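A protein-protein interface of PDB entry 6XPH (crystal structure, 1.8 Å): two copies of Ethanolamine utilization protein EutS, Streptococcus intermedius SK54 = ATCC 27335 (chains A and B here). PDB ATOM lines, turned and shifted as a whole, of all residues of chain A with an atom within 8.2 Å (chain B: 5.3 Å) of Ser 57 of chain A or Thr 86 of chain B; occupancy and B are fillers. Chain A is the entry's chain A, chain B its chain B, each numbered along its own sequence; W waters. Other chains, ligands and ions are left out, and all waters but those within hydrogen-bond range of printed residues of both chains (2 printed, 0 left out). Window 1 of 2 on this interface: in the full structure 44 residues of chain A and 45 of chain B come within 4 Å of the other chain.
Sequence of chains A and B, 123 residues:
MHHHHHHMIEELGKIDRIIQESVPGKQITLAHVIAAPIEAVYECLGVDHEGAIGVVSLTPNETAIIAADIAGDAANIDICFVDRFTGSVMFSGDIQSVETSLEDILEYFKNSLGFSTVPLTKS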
ATOM      1  N   THR A  29     -12.496   0.269  -7.651  1.00  0.00           N
ATOM      2  CA  THR A  29     -11.851   0.926  -8.813  1.00  0.00           C
ATOM      3  C   THR A  29     -12.922   1.304  -9.811  1.00  0.00           C
ATOM      4  O   THR A  29     -12.605   2.069 -10.763  1.00  0.00           O
ATOM      5  CB  THR A  29     -10.805   0.049  -9.478  1.00  0.00           C
ATOM      6  OG1 THR A  29     -11.422  -1.181  -9.871  1.00  0.00           O
ATOM      7  CG2 THR A  29      -9.606  -0.210  -8.581  1.00  0.00           C
ATOM      8  N   GLY A  54     -14.554  -9.285 -26.804  1.00  0.00           N
ATOM      9  CA  GLY A  54     -13.494  -9.801 -25.916  1.00  0.00           C
ATOM     10  C   GLY A  54     -13.283  -8.861 -24.755  1.00  0.00           C
ATOM     11  O   GLY A  54     -13.366  -7.621 -24.917  1.00  0.00           O
ATOM     12  N   VAL A  55     -13.096  -9.449 -23.575  1.00  0.00           N
ATOM     13  CA  VAL A  55     -12.819  -8.701 -22.328  1.00  0.00           C
ATOM     14  C   VAL A  55     -11.627  -9.333 -21.646  1.00  0.00           C
ATOM     15  O   VAL A  55     -11.606 -10.580 -21.492  1.00  0.00           O
ATOM     16  CB  VAL A  55     -14.013  -8.725 -21.362  1.00  0.00           C
ATOM     17  CG1 VAL A  55     -13.723  -7.910 -20.112  1.00  0.00           C
ATOM     18  CG2 VAL A  55     -15.303  -8.320 -22.059  1.00  0.00           C
ATOM     19  N   VAL A  56     -10.658  -8.486 -21.288  1.00  0.00           N
ATOM     20  CA  VAL A  56      -9.521  -8.936 -20.480  1.00  0.00           C
ATOM     21  C   VAL A  56      -9.451  -8.127 -19.202  1.00  0.00           C
ATOM     22  O   VAL A  56      -9.655  -6.895 -19.248  1.00  0.00           O
ATOM     23  CB  VAL A  56      -8.226  -8.835 -21.270  1.00  0.00           C
ATOM     24  CG1 VAL A  56      -7.014  -9.110 -20.428  1.00  0.00           C
ATOM     25  CG2 VAL A  56      -8.264  -9.788 -22.450  1.00  0.00           C
ATOM     26  N   SER A  57      -9.152  -8.798 -18.112  1.00  0.00           N
ATOM     27  CA  SER A  57      -8.836  -8.082 -16.855  1.00  0.00           C
ATOM     28  C   SER A  57      -7.516  -8.629 -16.336  1.00  0.00           C
ATOM     29  O   SER A  57      -7.258  -9.842 -16.520  1.00  0.00           O
ATOM     30  CB  SER A  57      -9.906  -8.247 -15.808  1.00  0.00           C
ATOM     31  OG  SER A  57     -11.125  -7.648 -16.217  1.00  0.00           O
ATOM     32  N   LEU A  58      -6.744  -7.758 -15.734  1.00  0.00           N
ATOM     33  CA  LEU A  58      -5.406  -8.144 -15.248  1.00  0.00           C
ATOM     34  C   LEU A  58      -4.881  -7.207 -14.198  1.00  0.00           C
ATOM     35  O   LEU A  58      -5.424  -6.160 -13.934  1.00  0.00           O
ATOM     36  CB  LEU A  58      -4.433  -8.175 -16.429  1.00  0.00           C
ATOM     37  CG  LEU A  58      -4.446  -7.021 -17.404  1.00  0.00           C
ATOM     38  CD1 LEU A  58      -4.117  -5.703 -16.744  1.00  0.00           C
ATOM     39  CD2 LEU A  58      -3.519  -7.329 -18.582  1.00  0.00           C
ATOM     40  N   THR A  59      -3.808  -7.670 -13.602  1.00  0.00           N
ATOM     41  CA  THR A  59      -3.124  -6.944 -12.521  1.00  0.00           C
ATOM     42  C   THR A  59      -1.642  -7.271 -12.671  1.00  0.00           C
ATOM     43  O   THR A  59      -1.285  -8.409 -12.993  1.00  0.00           O
ATOM     44  CB  THR A  59      -3.705  -7.297 -11.146  1.00  0.00           C
ATOM     45  OG1 THR A  59      -3.137  -6.309 -10.295  1.00  0.00           O
ATOM     46  CG2 THR A  59      -3.421  -8.716 -10.706  1.00  0.00           C
ATOM     47  N   PRO A  60      -0.750  -6.257 -12.533  1.00  0.00           N
ATOM     48  CA  PRO A  60      -1.083  -4.870 -12.218  1.00  0.00           C
ATOM     49  C   PRO A  60      -1.842  -4.116 -13.324  1.00  0.00           C
ATOM     50  O   PRO A  60      -1.710  -4.395 -14.522  1.00  0.00           O
ATOM     51  CB  PRO A  60       0.283  -4.188 -12.004  1.00  0.00           C
ATOM     52  CG  PRO A  60       1.259  -5.065 -12.685  1.00  0.00           C
ATOM     53  CD  PRO A  60       0.704  -6.477 -12.555  1.00  0.00           C
ATOM     54  N   ASN A  61      -2.790  -3.258 -12.883  1.00  0.00           N
ATOM     55  CA  ASN A  61      -3.853  -2.695 -13.761  1.00  0.00           C
ATOM     56  C   ASN A  61      -3.268  -1.893 -14.961  1.00  0.00           C
ATOM     57  O   ASN A  61      -3.810  -1.914 -16.050  1.00  0.00           O
ATOM     58  CB  ASN A  61      -4.754  -1.832 -12.871  1.00  0.00           C
ATOM     59  CG  ASN A  61      -5.641  -2.640 -11.925  1.00  0.00           C
ATOM     60  OD1 ASN A  61      -5.509  -3.862 -11.841  1.00  0.00           O
ATOM     61  ND2 ASN A  61      -6.556  -1.998 -11.188  1.00  0.00           N
ATOM     62  N   THR A  63      -0.917  -2.458 -16.909  1.00  0.00           N
ATOM     63  CA  THR A  63      -0.539  -3.303 -18.068  1.00  0.00           C
ATOM     64  C   THR A  63      -1.732  -3.522 -18.999  1.00  0.00           C
ATOM     65  O   THR A  63      -1.518  -4.072 -20.094  1.00  0.00           O
ATOM     66  CB  THR A  63       0.138  -4.613 -17.627  1.00  0.00           C
ATOM     67  OG1 THR A  63      -0.843  -5.420 -16.997  1.00  0.00           O
ATOM     68  CG2 THR A  63       1.343  -4.336 -16.758  1.00  0.00           C
ATOM     69  N   ALA A  64      -2.915  -2.986 -18.704  1.00  0.00           N
ATOM     70  CA  ALA A  64      -4.064  -3.134 -19.627  1.00  0.00           C
ATOM     71  C   ALA A  64      -3.691  -2.667 -21.031  1.00  0.00           C
ATOM     72  O   ALA A  64      -4.190  -3.210 -22.022  1.00  0.00           O
ATOM     73  CB  ALA A  64      -5.285  -2.398 -19.108  1.00  0.00           C
ATOM     74  N   ALA A  67      -2.300  -5.296 -23.369  1.00  0.00           N
ATOM     75  CA  ALA A  67      -3.373  -6.158 -23.915  1.00  0.00           C
ATOM     76  C   ALA A  67      -4.082  -5.432 -25.083  1.00  0.00           C
ATOM     77  O   ALA A  67      -4.351  -6.034 -26.122  1.00  0.00           O
ATOM     78  CB  ALA A  67      -4.295  -6.522 -22.821  1.00  0.00           C
ATOM     79  N   PHE A  81     -12.707  -0.041 -25.246  1.00  0.00           N
ATOM     80  CA  PHE A  81     -12.126   0.809 -24.200  1.00  0.00           C
ATOM     81  C   PHE A  81     -10.932   0.102 -23.557  1.00  0.00           C
ATOM     82  O   PHE A  81     -10.822  -1.127 -23.587  1.00  0.00           O
ATOM     83  CB  PHE A  81     -13.153   1.188 -23.127  1.00  0.00           C
ATOM     84  CG  PHE A  81     -13.537   0.099 -22.160  1.00  0.00           C
ATOM     85  CD1 PHE A  81     -12.693  -0.228 -21.109  1.00  0.00           C
ATOM     86  CD2 PHE A  81     -14.706  -0.614 -22.320  1.00  0.00           C
ATOM     87  CE1 PHE A  81     -13.027  -1.214 -20.205  1.00  0.00           C
ATOM     88  CE2 PHE A  81     -15.059  -1.599 -21.415  1.00  0.00           C
ATOM     89  CZ  PHE A  81     -14.211  -1.928 -20.374  1.00  0.00           C
ATOM     90  N   ASP A  83      -8.842   0.616 -19.776  1.00  0.00           N
ATOM     91  CA  ASP A  83      -8.931   1.289 -18.472  1.00  0.00           C
ATOM     92  C   ASP A  83      -7.730   0.836 -17.647  1.00  0.00           C
ATOM     93  O   ASP A  83      -7.751  -0.260 -17.118  1.00  0.00           O
ATOM     94  CB  ASP A  83     -10.284   1.047 -17.802  1.00  0.00           C
ATOM     95  CG  ASP A  83     -10.507   1.908 -16.563  1.00  0.00           C
ATOM     96  OD1 ASP A  83      -9.502   2.345 -15.883  1.00  0.00           O
ATOM     97  OD2 ASP A  83     -11.674   2.106 -16.231  1.00  0.00           O
ATOM     98  N   THR A  86      -8.661   0.332 -13.709  1.00  0.00           N
ATOM     99  CA  THR A  86      -9.410  -0.889 -13.319  1.00  0.00           C
ATOM    100  C   THR A  86      -8.652  -2.132 -13.797  1.00  0.00           C
ATOM    101  O   THR A  86      -8.958  -3.215 -13.313  1.00  0.00           O
ATOM    102  CB  THR A  86     -10.825  -0.817 -13.906  1.00  0.00           C
ATOM    103  OG1 THR A  86     -10.769  -0.786 -15.330  1.00  0.00           O
ATOM    104  CG2 THR A  86     -11.540   0.437 -13.450  1.00  0.00           C
ATOM    105  N   GLY A  87      -7.742  -1.947 -14.760  1.00  0.00           N
ATOM    106  CA  GLY A  87      -6.990  -3.042 -15.402  1.00  0.00           C
ATOM    107  C   GLY A  87      -7.843  -3.865 -16.343  1.00  0.00           C
ATOM    108  O   GLY A  87      -7.825  -5.133 -16.262  1.00  0.00           O
ATOM    109  N   SER A  88      -8.584  -3.220 -17.223  1.00  0.00           N
ATOM    110  CA  SER A  88      -9.499  -3.934 -18.129  1.00  0.00           C
ATOM    111  C   SER A  88      -9.427  -3.405 -19.534  1.00  0.00           C
ATOM    112  O   SER A  88      -9.187  -2.217 -19.785  1.00  0.00           O
ATOM    113  CB  SER A  88     -10.930  -3.780 -17.620  1.00  0.00           C
ATOM    114  OG  SER A  88     -11.056  -4.531 -16.409  1.00  0.00           O
ATOM    115  N   VAL A  89      -9.725  -4.272 -20.476  1.00  0.00           N
ATOM    116  CA  VAL A  89      -9.840  -3.851 -21.897  1.00  0.00           C
ATOM    117  C   VAL A  89     -11.018  -4.619 -22.506  1.00  0.00           C
ATOM    118  O   VAL A  89     -11.228  -5.790 -22.174  1.00  0.00           O
ATOM    119  CB  VAL A  89      -8.523  -4.018 -22.692  1.00  0.00           C
ATOM    120  CG1 VAL A  89      -7.957  -5.426 -22.657  1.00  0.00           C
ATOM    121  CG2 VAL A  89      -8.670  -3.548 -24.128  1.00  0.00           C
ATOM    122  N   MET A  90     -11.756  -3.940 -23.371  1.00  0.00           N
ATOM    123  CA  MET A  90     -12.857  -4.555 -24.106  1.00  0.00           C
ATOM    124  C   MET A  90     -12.627  -4.260 -25.566  1.00  0.00           C
ATOM    125  O   MET A  90     -12.283  -3.129 -25.901  1.00  0.00           O
ATOM    126  CB  MET A  90     -14.234  -4.051 -23.654  1.00  0.00           C
ATOM    127  CG  MET A  90     -15.300  -4.696 -24.406  1.00  0.00           C
ATOM    128  SD  MET A  90     -16.927  -4.168 -23.745  1.00  0.00           S
ATOM    129  CE  MET A  90     -16.850  -4.831 -22.089  1.00  0.00           C
ATOM    130  N   LEU A 102      -7.408 -13.045 -27.836  1.00  0.00           N
ATOM    131  CA  LEU A 102      -7.354 -13.445 -26.424  1.00  0.00           C
ATOM    132  C   LEU A 102      -6.206 -14.433 -26.210  1.00  0.00           C
ATOM    133  O   LEU A 102      -5.504 -14.306 -25.204  1.00  0.00           O
ATOM    134  CB  LEU A 102      -8.667 -14.055 -25.974  1.00  0.00           C
ATOM    135  CG  LEU A 102      -9.839 -13.090 -25.857  1.00  0.00           C
ATOM    136  CD1 LEU A 102     -11.128 -13.889 -25.601  1.00  0.00           C
ATOM    137  CD2 LEU A 102      -9.605 -12.084 -24.759  1.00  0.00           C
ATOM    138  N   ILE A 105      -2.889 -12.571 -26.245  1.00  0.00           N
ATOM    139  CA  ILE A 105      -2.718 -11.879 -24.942  1.00  0.00           C
ATOM    140  C   ILE A 105      -2.258 -12.865 -23.868  1.00  0.00           C
ATOM    141  O   ILE A 105      -1.292 -12.566 -23.144  1.00  0.00           O
ATOM    142  CB  ILE A 105      -4.022 -11.144 -24.579  1.00  0.00           C
ATOM    143  CG1 ILE A 105      -4.262  -9.998 -25.565  1.00  0.00           C
ATOM    144  CG2 ILE A 105      -3.979 -10.660 -23.179  1.00  0.00           C
ATOM    145  CD1 ILE A 105      -5.622  -9.381 -25.471  1.00  0.00           C
ATOM    146  N   LEU A 106      -2.961 -13.975 -23.685  1.00  0.00           N
ATOM    147  CA  LEU A 106      -2.592 -14.981 -22.659  1.00  0.00           C
ATOM    148  C   LEU A 106      -1.137 -15.402 -22.893  1.00  0.00           C
ATOM    149  O   LEU A 106      -0.365 -15.435 -21.908  1.00  0.00           O
ATOM    150  CB  LEU A 106      -3.572 -16.157 -22.755  1.00  0.00           C
ATOM    151  CG  LEU A 106      -4.965 -15.844 -22.211  1.00  0.00           C
ATOM    152  CD1 LEU A 106      -5.944 -16.909 -22.650  1.00  0.00           C
ATOM    153  CD2 LEU A 106      -4.993 -15.676 -20.728  1.00  0.00           C
ATOM    154  N   PHE A 109       1.565 -12.467 -22.126  1.00  0.00           N
ATOM    155  CA  PHE A 109       1.645 -12.143 -20.707  1.00  0.00           C
ATOM    156  C   PHE A 109       2.330 -13.286 -19.939  1.00  0.00           C
ATOM    157  O   PHE A 109       3.156 -13.001 -19.076  1.00  0.00           O
ATOM    158  CB  PHE A 109       0.282 -11.743 -20.140  1.00  0.00           C
ATOM    159  CG  PHE A 109      -0.012 -10.271 -20.340  1.00  0.00           C
ATOM    160  CD1 PHE A 109      -0.511  -9.789 -21.532  1.00  0.00           C
ATOM    161  CD2 PHE A 109       0.309  -9.355 -19.337  1.00  0.00           C
ATOM    162  CE1 PHE A 109      -0.857  -8.445 -21.680  1.00  0.00           C
ATOM    163  CE2 PHE A 109       0.044  -7.995 -19.525  1.00  0.00           C
ATOM    164  CZ  PHE A 109      -0.483  -7.547 -20.705  1.00  0.00           C
ATOM    165  N   PHE A 115       3.319 -13.640 -16.138  1.00  0.00           N
ATOM    166  CA  PHE A 115       1.980 -13.590 -15.507  1.00  0.00           C
ATOM    167  C   PHE A 115       1.384 -14.997 -15.388  1.00  0.00           C
ATOM    168  O   PHE A 115       1.594 -15.853 -16.279  1.00  0.00           O
ATOM    169  CB  PHE A 115       0.968 -12.743 -16.297  1.00  0.00           C
ATOM    170  CG  PHE A 115       1.069 -11.252 -16.130  1.00  0.00           C
ATOM    171  CD1 PHE A 115       2.294 -10.602 -16.221  1.00  0.00           C
ATOM    172  CD2 PHE A 115      -0.079 -10.485 -15.952  1.00  0.00           C
ATOM    173  CE1 PHE A 115       2.395  -9.232 -16.076  1.00  0.00           C
ATOM    174  CE2 PHE A 115       0.025  -9.120 -15.762  1.00  0.00           C
ATOM    175  CZ  PHE A 115       1.246  -8.492 -15.864  1.00  0.00           C
ATOM    176  N   SER A 116       0.672 -15.224 -14.302  1.00  0.00           N
ATOM    177  CA  SER A 116      -0.229 -16.392 -14.190  1.00  0.00           C
ATOM    178  C   SER A 116      -1.445 -16.084 -15.062  1.00  0.00           C
ATOM    179  O   SER A 116      -1.743 -14.885 -15.240  1.00  0.00           O
ATOM    180  CB  SER A 116      -0.602 -16.687 -12.751  1.00  0.00           C
ATOM    181  OG  SER A 116      -1.370 -15.639 -12.215  1.00  0.00           O
ATOM    182  N   THR A 117      -2.101 -17.116 -15.580  1.00  0.00           N
ATOM    183  CA  THR A 117      -3.263 -16.946 -16.487  1.00  0.00           C
ATOM    184  C   THR A 117      -4.428 -17.835 -16.050  1.00  0.00           C
ATOM    185  O   THR A 117      -4.249 -18.868 -15.424  1.00  0.00           O
ATOM    186  CB  THR A 117      -2.840 -17.195 -17.941  1.00  0.00           C
ATOM    187  OG1 THR A 117      -2.299 -18.512 -17.864  1.00  0.00           O
ATOM    188  CG2 THR A 117      -1.811 -16.201 -18.445  1.00  0.00           C
ATOM    189  N   VAL A 118      -5.583 -17.447 -16.511  1.00  0.00           N
ATOM    190  CA  VAL A 118      -6.858 -18.180 -16.422  1.00  0.00           C
ATOM    191  C   VAL A 118      -7.104 -18.852 -17.756  1.00  0.00           C
ATOM    192  O   VAL A 118      -6.598 -18.473 -18.817  1.00  0.00           O
ATOM    193  CB  VAL A 118      -8.012 -17.239 -16.020  1.00  0.00           C
ATOM    194  CG1 VAL A 118      -7.896 -16.791 -14.574  1.00  0.00           C
ATOM    195  CG2 VAL A 118      -8.125 -15.994 -16.915  1.00  0.00           C
ATOM    196  N   GLN B  27      -1.123 -11.211 -12.890  1.00  0.00           N
ATOM    197  CA  GLN B  27      -2.181 -12.200 -13.205  1.00  0.00           C
ATOM    198  C   GLN B  27      -3.050 -11.666 -14.323  1.00  0.00           C
ATOM    199  O   GLN B  27      -3.432 -10.487 -14.279  1.00  0.00           O
ATOM    200  CB  GLN B  27      -3.074 -12.465 -11.971  1.00  0.00           C
ATOM    201  CG  GLN B  27      -2.348 -12.672 -10.672  1.00  0.00           C
ATOM    202  CD  GLN B  27      -3.274 -13.226  -9.607  1.00  0.00           C
ATOM    203  OE1 GLN B  27      -3.000 -14.267  -9.002  1.00  0.00           O
ATOM    204  NE2 GLN B  27      -4.372 -12.536  -9.350  1.00  0.00           N
ATOM    205  N   ILE B  28      -3.347 -12.485 -15.309  1.00  0.00           N
ATOM    206  CA  ILE B  28      -4.565 -12.291 -16.127  1.00  0.00           C
ATOM    207  C   ILE B  28      -5.693 -13.004 -15.375  1.00  0.00           C
ATOM    208  O   ILE B  28      -5.584 -14.213 -15.127  1.00  0.00           O
ATOM    209  CB  ILE B  28      -4.381 -12.784 -17.563  1.00  0.00           C
ATOM    210  CG1 ILE B  28      -3.351 -11.934 -18.320  1.00  0.00           C
ATOM    211  CG2 ILE B  28      -5.710 -12.835 -18.262  1.00  0.00           C
ATOM    212  CD1 ILE B  28      -3.321 -12.178 -19.794  1.00  0.00           C
ATOM    213  N   THR B  29      -6.672 -12.246 -14.948  1.00  0.00           N
ATOM    214  CA  THR B  29      -7.768 -12.756 -14.094  1.00  0.00           C
ATOM    215  C   THR B  29      -8.995 -13.001 -14.975  1.00  0.00           C
ATOM    216  O   THR B  29      -9.882 -13.714 -14.486  1.00  0.00           O
ATOM    217  CB  THR B  29      -8.115 -11.759 -12.966  1.00  0.00           C
ATOM    218  OG1 THR B  29      -8.537 -10.528 -13.575  1.00  0.00           O
ATOM    219  CG2 THR B  29      -6.979 -11.496 -12.000  1.00  0.00           C
ATOM    220  N   LEU B  30      -9.090 -12.485 -16.218  1.00  0.00           N
ATOM    221  CA  LEU B  30     -10.238 -12.726 -17.106  1.00  0.00           C
ATOM    222  C   LEU B  30      -9.757 -12.606 -18.538  1.00  0.00           C
ATOM    223  O   LEU B  30      -9.047 -11.653 -18.838  1.00  0.00           O
ATOM    224  CB  LEU B  30     -11.361 -11.743 -16.819  1.00  0.00           C
ATOM    225  CG  LEU B  30     -12.628 -11.986 -17.621  1.00  0.00           C
ATOM    226  CD1 LEU B  30     -13.332 -13.261 -17.184  1.00  0.00           C
ATOM    227  CD2 LEU B  30     -13.539 -10.786 -17.450  1.00  0.00           C
ATOM    228  N   ALA B  31     -10.080 -13.599 -19.393  1.00  0.00           N
ATOM    229  CA  ALA B  31      -9.819 -13.533 -20.823  1.00  0.00           C
ATOM    230  C   ALA B  31     -11.015 -14.191 -21.496  1.00  0.00           C
ATOM    231  O   ALA B  31     -11.048 -15.419 -21.573  1.00  0.00           O
ATOM    232  CB  ALA B  31      -8.518 -14.211 -21.148  1.00  0.00           C
ATOM    233  N   LEU B  58     -13.292  -4.155  -7.851  1.00  0.00           N
ATOM    234  CA  LEU B  58     -12.605  -3.837  -6.599  1.00  0.00           C
ATOM    235  C   LEU B  58     -11.434  -4.756  -6.326  1.00  0.00           C
ATOM    236  O   LEU B  58     -11.300  -5.798  -6.979  1.00  0.00           O
ATOM    237  CB  LEU B  58     -13.589  -3.801  -5.443  1.00  0.00           C
ATOM    238  CG  LEU B  58     -14.550  -4.960  -5.310  1.00  0.00           C
ATOM    239  CD1 LEU B  58     -13.813  -6.237  -5.007  1.00  0.00           C
ATOM    240  CD2 LEU B  58     -15.599  -4.649  -4.266  1.00  0.00           C
ATOM    241  N   ASN B  61      -9.747  -8.870  -4.617  1.00  0.00           N
ATOM    242  CA  ASN B  61     -10.787  -9.323  -5.582  1.00  0.00           C
ATOM    243  C   ASN B  61     -11.864 -10.161  -4.859  1.00  0.00           C
ATOM    244  O   ASN B  61     -13.034 -10.134  -5.321  1.00  0.00           O
ATOM    245  CB  ASN B  61     -10.155 -10.029  -6.803  1.00  0.00           C
ATOM    246  CG  ASN B  61      -9.246  -9.147  -7.654  1.00  0.00           C
ATOM    247  OD1 ASN B  61      -9.145  -7.938  -7.432  1.00  0.00           O
ATOM    248  ND2 ASN B  61      -8.549  -9.724  -8.644  1.00  0.00           N
ATOM    249  N   ASP B  83     -17.596 -12.408 -10.039  1.00  0.00           N
ATOM    250  CA  ASP B  83     -16.333 -13.138 -10.286  1.00  0.00           C
ATOM    251  C   ASP B  83     -15.337 -12.751  -9.177  1.00  0.00           C
ATOM    252  O   ASP B  83     -14.757 -11.633  -9.188  1.00  0.00           O
ATOM    253  CB  ASP B  83     -15.888 -12.921 -11.730  1.00  0.00           C
ATOM    254  CG  ASP B  83     -14.607 -13.685 -12.102  1.00  0.00           C
ATOM    255  OD1 ASP B  83     -13.796 -14.042 -11.188  1.00  0.00           O
ATOM    256  OD2 ASP B  83     -14.361 -13.789 -13.316  1.00  0.00           O
ATOM    257  N   ARG B  84     -15.167 -13.640  -8.186  1.00  0.00           N
ATOM    258  CA  ARG B  84     -14.316 -13.406  -7.007  1.00  0.00           C
ATOM    259  C   ARG B  84     -12.861 -13.314  -7.458  1.00  0.00           C
ATOM    260  O   ARG B  84     -12.044 -12.816  -6.724  1.00  0.00           O
ATOM    261  CB  ARG B  84     -14.497 -14.524  -5.980  1.00  0.00           C
ATOM    262  CG  ARG B  84     -15.875 -14.506  -5.342  1.00  0.00           C
ATOM    263  CD  ARG B  84     -16.075 -15.876  -4.791  1.00  0.00           C
ATOM    264  NE  ARG B  84     -17.154 -16.119  -3.880  1.00  0.00           N
ATOM    265  CZ  ARG B  84     -18.325 -16.583  -4.221  1.00  0.00           C
ATOM    266  NH1 ARG B  84     -18.696 -16.641  -5.493  1.00  0.00           N
ATOM    267  NH2 ARG B  84     -19.175 -16.890  -3.261  1.00  0.00           N
ATOM    268  N   PHE B  85     -12.503 -13.996  -8.521  1.00  0.00           N
ATOM    269  CA  PHE B  85     -11.074 -14.033  -8.925  1.00  0.00           C
ATOM    270  C   PHE B  85     -10.682 -12.734  -9.603  1.00  0.00           C
ATOM    271  O   PHE B  85      -9.572 -12.233  -9.420  1.00  0.00           O
ATOM    272  CB  PHE B  85     -10.784 -15.175  -9.896  1.00  0.00           C
ATOM    273  CG  PHE B  85      -9.310 -15.446 -10.001  1.00  0.00           C
ATOM    274  CD1 PHE B  85      -8.624 -15.998  -8.935  1.00  0.00           C
ATOM    275  CD2 PHE B  85      -8.624 -15.188 -11.190  1.00  0.00           C
ATOM    276  CE1 PHE B  85      -7.256 -16.226  -9.037  1.00  0.00           C
ATOM    277  CE2 PHE B  85      -7.270 -15.444 -11.300  1.00  0.00           C
ATOM    278  CZ  PHE B  85      -6.592 -15.988 -10.226  1.00  0.00           C
ATOM    279  N   THR B  86     -11.596 -12.131 -10.361  1.00  0.00           N
ATOM    280  CA  THR B  86     -11.343 -10.876 -11.090  1.00  0.00           C
ATOM    281  C   THR B  86     -11.716  -9.655 -10.226  1.00  0.00           C
ATOM    282  O   THR B  86     -11.190  -8.540 -10.473  1.00  0.00           O
ATOM    283  CB  THR B  86     -12.090 -10.970 -12.428  1.00  0.00           C
ATOM    284  OG1 THR B  86     -11.261 -10.178 -13.260  1.00  0.00           O
ATOM    285  CG2 THR B  86     -13.510 -10.492 -12.261  1.00  0.00           C
ATOM    286  N   GLY B  87     -12.566  -9.843  -9.207  1.00  0.00           N
ATOM    287  CA  GLY B  87     -13.035  -8.731  -8.380  1.00  0.00           C
ATOM    288  C   GLY B  87     -14.124  -7.898  -9.038  1.00  0.00           C
ATOM    289  O   GLY B  87     -14.151  -6.695  -8.832  1.00  0.00           O
ATOM    290  N   SER B  88     -15.015  -8.508  -9.808  1.00  0.00           N
ATOM    291  CA  SER B  88     -16.035  -7.758 -10.541  1.00  0.00           C
ATOM    292  C   SER B  88     -17.425  -8.316 -10.253  1.00  0.00           C
ATOM    293  O   SER B  88     -17.579  -9.551 -10.104  1.00  0.00           O
ATOM    294  CB  SER B  88     -15.773  -7.793 -12.027  1.00  0.00           C
ATOM    295  OG  SER B  88     -14.554  -7.108 -12.255  1.00  0.00           O
HETATM  296  O   HOH W   1      -4.235 -15.706 -13.121  1.00  0.00           O
HETATM  297  O   HOH W   2     -12.355  -7.880 -13.869  1.00  0.00           O
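Among the printed residues, merely in contact across the chains: Val 56 of chain A with Leu 30 of chain B, Leu 58 of chain A with Gln 27 of chain B, Phe 115 of chain A with Gln 27 of chain B, Ser 116 of chain A with Gln 27 of chain B, Ser 57 of chain A with Thr 86 of chain B, Val 118 of chain A with Ile 28 of chain B, Val 55 of chain A with Ala 31 of chain B, Val 118 of chain A with Phe 85 of chain B, Phe 109 of chain A with Ile 28 of chain B, Ser 57 of chain A with Ile 28 of chain B, Val 118 of chain A with Thr 29 of chain B, Val 118 of chain A with Leu 30 of chain B, Ile 105 of chain A with Ile 28 of chain B, Leu 106 of chain A with Ile 28 of chain B, Thr 117 of chain A with Ile 28 of chain B, Val 55 of chain A with Leu 30 of chain B, Leu 106 of chain A with Ala 31 of chain B, Phe 115 of chain A with Ile 28 of chain B, Leu 58 of chain A with Thr 29 of chain B and Val 118 of chain A with Ala 31 of chain B.
The backbone NH of Thr 29 of chain B sits at hydrogen-bond distance from the backbone carbonyl oxygen of Ser 57 of chain A.
The backbone carbonyl oxygen of Leu 30 of chain B lies within hydrogen-bond range of the backbone NH of Ser 57 of chain A.
O of Thr 59 of chain A sits at hydrogen-bond distance from N of Gln 27 of chain B, 2.8 Å away.
The backbone NH (N) of Ile 28 of chain B sits at hydrogen-bond distance from the backbone carbonyl oxygen (O) of Ser 116 of chain A (2.9 Å).
OG of Ser 88 of chain A lies within hydrogen-bond range of OG of Ser 57 of chain A, at 3.1 Å.
The backbone carbonyl oxygen (O) of Gly 87 of chain A sits at hydrogen-bond distance from the backbone NH (N) of Leu 58 of chain A.
N of Phe 85 of chain B sits at hydrogen-bond distance from OD1 of Asp 83 of chain B, at 3.0 Å.
Of the printed residues of chain B, Ser 57 of chain A touches Ile 28 (3.7 Å), Thr 29 (2.9 Å), Leu 30 (2.9 Å) and Thr 86 (3.5 Å).
Of the printed residues of chain A, Ile 28 of chain B touches Ser 57, Ile 105, Leu 106, Phe 109, Phe 115, Ser 116, Thr 117 and Val 118.
The nearest printed residue of chain B that does not touch Ser 57 of chain A is Gln 27 of chain B (4.5 Å).
The nearest printed residue of chain A that does not touch Thr 86 of chain B is Leu 58 of chain A (5.7 Å).
The nearest printed residue of chain B that does not touch Leu 106 of chain A is Leu 30 of chain B (6.0 Å).
Leu 58 of chain A touches Thr 29 of chain B, but with the chains exchanged Thr 29 of chain A does not touch Leu 58 of chain B (4.1 Å).
Of the 24 pairs that touch across the chains among the printed residues, none has its exchanged pair printed and touching as well.
Water W2 lies within hydrogen-bond range of the side-chain hydroxyl of Thr 86 of chain B, the side-chain hydroxyl of Ser 57 of chain A and the side-chain hydroxyl of Ser 88 of chain B.
Water W1 bridges O of Ile 28 of chain B (2.8 Å) and OG of Ser 116 of chain A (3.0 Å).
Of the 13 printed residues of chain B, 7 touch a printed residue of chain A.
Hydrophobic or aromatic side chains of chain B that line the printed part of chain A: Ile 28, Leu 30, Ala 31 and Phe 85.
Along chain B the printed residues that touch a printed residue of chain A span positions 27 to 86.
Of the 27 printed residues of chain A, 12 touch a printed residue of chain B.
Printed residues of chain A that touch a printed residue of chain B: Val 55, Val 56, Ser 57, Leu 58, Thr 59, Ile 105, Leu 106, Phe 109, Phe 115, Ser 116, Thr 117 and Val 118.
Among the printed residues, 24 pairs touch across the chains.
Among the printed residues, no Asp or Glu carboxylate lies within 4 Å of a Lys or Arg side-chain nitrogen of the other chain.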
